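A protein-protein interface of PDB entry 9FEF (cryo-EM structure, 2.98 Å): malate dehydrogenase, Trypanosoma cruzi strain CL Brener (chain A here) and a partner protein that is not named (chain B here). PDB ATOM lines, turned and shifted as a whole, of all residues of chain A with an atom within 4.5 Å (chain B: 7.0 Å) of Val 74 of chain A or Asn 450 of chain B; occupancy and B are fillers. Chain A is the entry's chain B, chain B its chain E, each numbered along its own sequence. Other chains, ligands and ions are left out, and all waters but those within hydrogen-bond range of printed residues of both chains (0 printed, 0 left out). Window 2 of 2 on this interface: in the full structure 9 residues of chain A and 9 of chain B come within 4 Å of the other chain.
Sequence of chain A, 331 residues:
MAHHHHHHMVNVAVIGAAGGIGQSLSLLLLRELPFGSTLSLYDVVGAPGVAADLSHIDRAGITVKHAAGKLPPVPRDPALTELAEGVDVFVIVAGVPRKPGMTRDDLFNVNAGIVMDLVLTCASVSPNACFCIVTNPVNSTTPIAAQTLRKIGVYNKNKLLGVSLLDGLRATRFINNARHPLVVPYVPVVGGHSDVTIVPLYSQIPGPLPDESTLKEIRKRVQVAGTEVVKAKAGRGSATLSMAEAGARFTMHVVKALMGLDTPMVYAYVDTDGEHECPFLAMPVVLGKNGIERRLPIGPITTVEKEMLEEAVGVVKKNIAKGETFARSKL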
ATOM      1  N   LYS A  70     -20.234  25.463  -2.382  1.00  0.00           N
ATOM      2  CA  LYS A  70     -20.769  24.171  -2.785  1.00  0.00           C
ATOM      3  C   LYS A  70     -19.825  23.579  -3.823  1.00  0.00           C
ATOM      4  O   LYS A  70     -18.846  24.210  -4.231  1.00  0.00           O
ATOM      5  CB  LYS A  70     -22.203  24.322  -3.320  1.00  0.00           C
ATOM      6  CG  LYS A  70     -22.978  23.028  -3.564  1.00  0.00           C
ATOM      7  CD  LYS A  70     -23.084  22.187  -2.301  1.00  0.00           C
ATOM      8  CE  LYS A  70     -23.677  22.978  -1.144  1.00  0.00           C
ATOM      9  NZ  LYS A  70     -24.022  22.101   0.010  1.00  0.00           N
ATOM     10  N   PRO A  72     -18.957  22.372  -7.711  1.00  0.00           N
ATOM     11  CA  PRO A  72     -19.006  23.288  -8.869  1.00  0.00           C
ATOM     12  C   PRO A  72     -20.390  23.877  -9.074  1.00  0.00           C
ATOM     13  O   PRO A  72     -21.394  23.149  -9.052  1.00  0.00           O
ATOM     14  CB  PRO A  72     -18.601  22.380 -10.034  1.00  0.00           C
ATOM     15  CG  PRO A  72     -17.619  21.432  -9.411  1.00  0.00           C
ATOM     16  CD  PRO A  72     -17.970  21.298  -7.936  1.00  0.00           C
ATOM     17  N   PRO A  73     -20.471  25.200  -9.294  1.00  0.00           N
ATOM     18  CA  PRO A  73     -21.689  25.961  -8.969  1.00  0.00           C
ATOM     19  C   PRO A  73     -23.001  25.375  -9.466  1.00  0.00           C
ATOM     20  O   PRO A  73     -23.109  24.920 -10.609  1.00  0.00           O
ATOM     21  CB  PRO A  73     -21.417  27.317  -9.629  1.00  0.00           C
ATOM     22  CG  PRO A  73     -19.941  27.461  -9.538  1.00  0.00           C
ATOM     23  CD  PRO A  73     -19.395  26.076  -9.787  1.00  0.00           C
ATOM     24  N   VAL A  74     -24.002  25.384  -8.592  1.00  0.00           N
ATOM     25  CA  VAL A  74     -25.351  24.938  -8.925  1.00  0.00           C
ATOM     26  C   VAL A  74     -26.278  26.148  -8.887  1.00  0.00           C
ATOM     27  O   VAL A  74     -26.085  27.050  -8.060  1.00  0.00           O
ATOM     28  CB  VAL A  74     -25.824  23.832  -7.966  1.00  0.00           C
ATOM     29  CG1 VAL A  74     -24.965  22.591  -8.132  1.00  0.00           C
ATOM     30  CG2 VAL A  74     -25.783  24.315  -6.526  1.00  0.00           C
ATOM     31  N   PRO A  75     -27.272  26.229  -9.771  1.00  0.00           N
ATOM     32  CA  PRO A  75     -28.201  27.364  -9.734  1.00  0.00           C
ATOM     33  C   PRO A  75     -29.039  27.369  -8.465  1.00  0.00           C
ATOM     34  O   PRO A  75     -29.434  26.318  -7.954  1.00  0.00           O
ATOM     35  CB  PRO A  75     -29.075  27.143 -10.976  1.00  0.00           C
ATOM     36  CG  PRO A  75     -28.986  25.680 -11.240  1.00  0.00           C
ATOM     37  CD  PRO A  75     -27.594  25.284 -10.854  1.00  0.00           C
ATOM     38  N   ARG A  76     -29.313  28.575  -7.967  1.00  0.00           N
ATOM     39  CA  ARG A  76     -30.142  28.784  -6.779  1.00  0.00           C
ATOM     40  C   ARG A  76     -29.602  27.992  -5.587  1.00  0.00           C
ATOM     41  O   ARG A  76     -30.243  27.077  -5.066  1.00  0.00           O
ATOM     42  CB  ARG A  76     -31.604  28.429  -7.067  1.00  0.00           C
ATOM     43  CG  ARG A  76     -32.194  29.164  -8.260  1.00  0.00           C
ATOM     44  CD  ARG A  76     -32.789  30.501  -7.855  1.00  0.00           C
ATOM     45  NE  ARG A  76     -33.470  30.431  -6.568  1.00  0.00           N
ATOM     46  CZ  ARG A  76     -34.784  30.511  -6.412  1.00  0.00           C
ATOM     47  NH1 ARG A  76     -35.595  30.663  -7.446  1.00  0.00           N
ATOM     48  NH2 ARG A  76     -35.297  30.435  -5.187  1.00  0.00           N
ATOM     49  N   ASP A  77     -28.397  28.363  -5.168  1.00  0.00           N
ATOM     50  CA  ASP A  77     -27.713  27.638  -4.106  1.00  0.00           C
ATOM     51  C   ASP A  77     -28.505  27.725  -2.805  1.00  0.00           C
ATOM     52  O   ASP A  77     -28.917  28.824  -2.409  1.00  0.00           O
ATOM     53  CB  ASP A  77     -26.309  28.204  -3.902  1.00  0.00           C
ATOM     54  CG  ASP A  77     -25.358  27.197  -3.295  1.00  0.00           C
ATOM     55  OD1 ASP A  77     -25.563  26.819  -2.123  1.00  0.00           O
ATOM     56  OD2 ASP A  77     -24.405  26.786  -3.987  1.00  0.00           O
ATOM     57  N   ALA B 442     -25.598  14.655 -19.845  1.00  0.00           N
ATOM     58  CA  ALA B 442     -24.492  15.599 -19.739  1.00  0.00           C
ATOM     59  C   ALA B 442     -24.739  16.838 -20.591  1.00  0.00           C
ATOM     60  O   ALA B 442     -24.473  17.965 -20.155  1.00  0.00           O
ATOM     61  CB  ALA B 442     -23.182  14.923 -20.139  1.00  0.00           C
ATOM     62  N   SER B 444     -27.659  18.086 -21.544  1.00  0.00           N
ATOM     63  CA  SER B 444     -28.722  18.871 -20.924  1.00  0.00           C
ATOM     64  C   SER B 444     -28.218  19.614 -19.693  1.00  0.00           C
ATOM     65  O   SER B 444     -28.580  20.774 -19.468  1.00  0.00           O
ATOM     66  CB  SER B 444     -29.899  17.966 -20.562  1.00  0.00           C
ATOM     67  OG  SER B 444     -30.529  17.460 -21.725  1.00  0.00           O
ATOM     68  N   HIS B 445     -27.388  18.959 -18.878  1.00  0.00           N
ATOM     69  CA  HIS B 445     -26.867  19.606 -17.678  1.00  0.00           C
ATOM     70  C   HIS B 445     -25.927  20.753 -18.030  1.00  0.00           C
ATOM     71  O   HIS B 445     -25.916  21.782 -17.347  1.00  0.00           O
ATOM     72  CB  HIS B 445     -26.166  18.578 -16.792  1.00  0.00           C
ATOM     73  CG  HIS B 445     -27.106  17.644 -16.096  1.00  0.00           C
ATOM     74  ND1 HIS B 445     -28.276  18.072 -15.503  1.00  0.00           N
ATOM     75  CD2 HIS B 445     -27.051  16.306 -15.896  1.00  0.00           C
ATOM     76  CE1 HIS B 445     -28.899  17.037 -14.970  1.00  0.00           C
ATOM     77  NE2 HIS B 445     -28.178  15.953 -15.194  1.00  0.00           N
ATOM     78  N   THR B 446     -25.124  20.593 -19.086  1.00  0.00           N
ATOM     79  CA  THR B 446     -24.293  21.703 -19.542  1.00  0.00           C
ATOM     80  C   THR B 446     -25.151  22.846 -20.067  1.00  0.00           C
ATOM     81  O   THR B 446     -24.805  24.020 -19.894  1.00  0.00           O
ATOM     82  CB  THR B 446     -23.315  21.231 -20.618  1.00  0.00           C
ATOM     83  OG1 THR B 446     -23.968  20.294 -21.482  1.00  0.00           O
ATOM     84  CG2 THR B 446     -22.109  20.565 -19.981  1.00  0.00           C
ATOM     85  N   ASN B 447     -26.271  22.521 -20.716  1.00  0.00           N
ATOM     86  CA  ASN B 447     -27.194  23.561 -21.160  1.00  0.00           C
ATOM     87  C   ASN B 447     -27.858  24.242 -19.967  1.00  0.00           C
ATOM     88  O   ASN B 447     -28.226  25.420 -20.041  1.00  0.00           O
ATOM     89  CB  ASN B 447     -28.242  22.955 -22.099  1.00  0.00           C
ATOM     90  CG  ASN B 447     -29.100  24.005 -22.796  1.00  0.00           C
ATOM     91  OD1 ASN B 447     -29.913  23.672 -23.659  1.00  0.00           O
ATOM     92  ND2 ASN B 447     -28.902  25.273 -22.454  1.00  0.00           N
ATOM     93  N   GLU B 448     -28.019  23.516 -18.862  1.00  0.00           N
ATOM     94  CA  GLU B 448     -28.688  24.028 -17.672  1.00  0.00           C
ATOM     95  C   GLU B 448     -27.728  24.711 -16.699  1.00  0.00           C
ATOM     96  O   GLU B 448     -28.158  25.138 -15.622  1.00  0.00           O
ATOM     97  CB  GLU B 448     -29.435  22.880 -16.976  1.00  0.00           C
ATOM     98  CG  GLU B 448     -30.467  23.299 -15.936  1.00  0.00           C
ATOM     99  CD  GLU B 448     -31.656  24.010 -16.549  1.00  0.00           C
ATOM    100  OE1 GLU B 448     -32.580  23.321 -17.029  1.00  0.00           O
ATOM    101  OE2 GLU B 448     -31.665  25.258 -16.550  1.00  0.00           O
ATOM    102  N   HIS B 449     -26.448  24.832 -17.058  1.00  0.00           N
ATOM    103  CA  HIS B 449     -25.427  25.440 -16.200  1.00  0.00           C
ATOM    104  C   HIS B 449     -25.263  24.681 -14.885  1.00  0.00           C
ATOM    105  O   HIS B 449     -24.980  25.278 -13.844  1.00  0.00           O
ATOM    106  CB  HIS B 449     -25.723  26.918 -15.923  1.00  0.00           C
ATOM    107  CG  HIS B 449     -26.013  27.721 -17.152  1.00  0.00           C
ATOM    108  ND1 HIS B 449     -27.256  27.748 -17.748  1.00  0.00           N
ATOM    109  CD2 HIS B 449     -25.224  28.532 -17.895  1.00  0.00           C
ATOM    110  CE1 HIS B 449     -27.218  28.538 -18.806  1.00  0.00           C
ATOM    111  NE2 HIS B 449     -25.996  29.027 -18.918  1.00  0.00           N
ATOM    112  N   ASN B 450     -25.439  23.362 -14.921  1.00  0.00           N
ATOM    113  CA  ASN B 450     -25.235  22.504 -13.754  1.00  0.00           C
ATOM    114  C   ASN B 450     -23.924  21.756 -13.960  1.00  0.00           C
ATOM    115  O   ASN B 450     -23.884  20.720 -14.628  1.00  0.00           O
ATOM    116  CB  ASN B 450     -26.409  21.549 -13.570  1.00  0.00           C
ATOM    117  CG  ASN B 450     -26.634  21.177 -12.119  1.00  0.00           C
ATOM    118  OD1 ASN B 450     -25.751  21.349 -11.279  1.00  0.00           O
ATOM    119  ND2 ASN B 450     -27.820  20.665 -11.816  1.00  0.00           N
ATOM    120  N   VAL B 451     -22.845  22.286 -13.380  1.00  0.00           N
ATOM    121  CA  VAL B 451     -21.516  21.739 -13.636  1.00  0.00           C
ATOM    122  C   VAL B 451     -21.357  20.373 -12.978  1.00  0.00           C
ATOM    123  O   VAL B 451     -20.827  19.433 -13.585  1.00  0.00           O
ATOM    124  CB  VAL B 451     -20.432  22.723 -13.163  1.00  0.00           C
ATOM    125  CG1 VAL B 451     -19.054  22.239 -13.590  1.00  0.00           C
ATOM    126  CG2 VAL B 451     -20.707  24.116 -13.707  1.00  0.00           C
ATOM    127  N   GLY B 452     -21.805  20.242 -11.729  1.00  0.00           N
ATOM    128  CA  GLY B 452     -21.639  18.982 -11.022  1.00  0.00           C
ATOM    129  C   GLY B 452     -22.414  17.841 -11.652  1.00  0.00           C
ATOM    130  O   GLY B 452     -21.891  16.733 -11.804  1.00  0.00           O
ATOM    131  N   ALA B 453     -23.671  18.093 -12.024  1.00  0.00           N
ATOM    132  CA  ALA B 453     -24.474  17.056 -12.662  1.00  0.00           C
ATOM    133  C   ALA B 453     -23.884  16.651 -14.007  1.00  0.00           C
ATOM    134  O   ALA B 453     -23.858  15.463 -14.349  1.00  0.00           O
ATOM    135  CB  ALA B 453     -25.915  17.537 -12.827  1.00  0.00           C
ATOM    136  N   ALA B 454     -23.408  17.625 -14.786  1.00  0.00           N
ATOM    137  CA  ALA B 454     -22.781  17.311 -16.065  1.00  0.00           C
ATOM    138  C   ALA B 454     -21.520  16.479 -15.873  1.00  0.00           C
ATOM    139  O   ALA B 454     -21.280  15.521 -16.618  1.00  0.00           O
ATOM    140  CB  ALA B 454     -22.464  18.597 -16.826  1.00  0.00           C
ATOM    141  N   LEU B 455     -20.699  16.833 -14.881  1.00  0.00           N
ATOM    142  CA  LEU B 455     -19.490  16.060 -14.610  1.00  0.00           C
ATOM    143  C   LEU B 455     -19.828  14.637 -14.183  1.00  0.00           C
ATOM    144  O   LEU B 455     -19.178  13.679 -14.616  1.00  0.00           O
ATOM    145  CB  LEU B 455     -18.650  16.758 -13.541  1.00  0.00           C
ATOM    146  CG  LEU B 455     -17.850  17.986 -13.982  1.00  0.00           C
ATOM    147  CD1 LEU B 455     -16.685  18.232 -13.039  1.00  0.00           C
ATOM    148  CD2 LEU B 455     -17.360  17.829 -15.415  1.00  0.00           C
ATOM    149  N   LEU B 531     -18.764  24.147 -20.853  1.00  0.00           N
ATOM    150  CA  LEU B 531     -19.220  24.655 -19.566  1.00  0.00           C
ATOM    151  C   LEU B 531     -18.074  25.092 -18.663  1.00  0.00           C
ATOM    152  O   LEU B 531     -18.331  25.630 -17.580  1.00  0.00           O
ATOM    153  CB  LEU B 531     -20.078  23.602 -18.859  1.00  0.00           C
ATOM    154  CG  LEU B 531     -19.407  22.595 -17.926  1.00  0.00           C
ATOM    155  CD1 LEU B 531     -20.441  21.971 -17.017  1.00  0.00           C
ATOM    156  CD2 LEU B 531     -18.703  21.520 -18.723  1.00  0.00           C
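The backbone carbonyl oxygen of His 445 of chain B sits at hydrogen-bond distance from the backbone NH of Asn 450 of chain B, 2.9 Å away. The backbone carbonyl oxygen (O) of Asn 447 of chain B sits at hydrogen-bond distance from a ring nitrogen (ND1) of His 449 of chain B.
Among the printed residues, pairs that only touch across the chains: Pro 72 of chain A with Val 451 of chain B, Pro 72 of chain A with Gly 452 of chain B, Pro 73 of chain A with His 449 of chain B, Pro 73 of chain A with Val 451 of chain B, Val 74 of chain A with Asn 450 of chain B and Pro 75 of chain A with His 449 of chain B.
Printed residues of chain B that touch a printed residue of chain A: His 449, Asn 450, Val 451 and Gly 452. Hydrophobic or aromatic side chains of chain B that line the printed part of chain A: Val 451. Of the 7 printed residues of chain A, 4 touch a printed residue of chain B.
Of the printed residues of chain B, Pro 73 of chain A touches His 449 and Val 451. Val 74 of chain A touches just one residue of chain B: Asn 450. Printed residues of chain B within 4 Å of Pro 75 of chain A: His 449. Thr 446 of chain B touches none of the printed residues of chain A. Of the printed residues of chain A, Asn 450 of chain B touches Val 74. The nearest residue of chain B that does not touch Val 74 of chain A is His 449 of chain B (4.9 Å). The nearest printed residue of chain A that does not touch Val 451 of chain B is Val 74 of chain A (5.7 Å).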
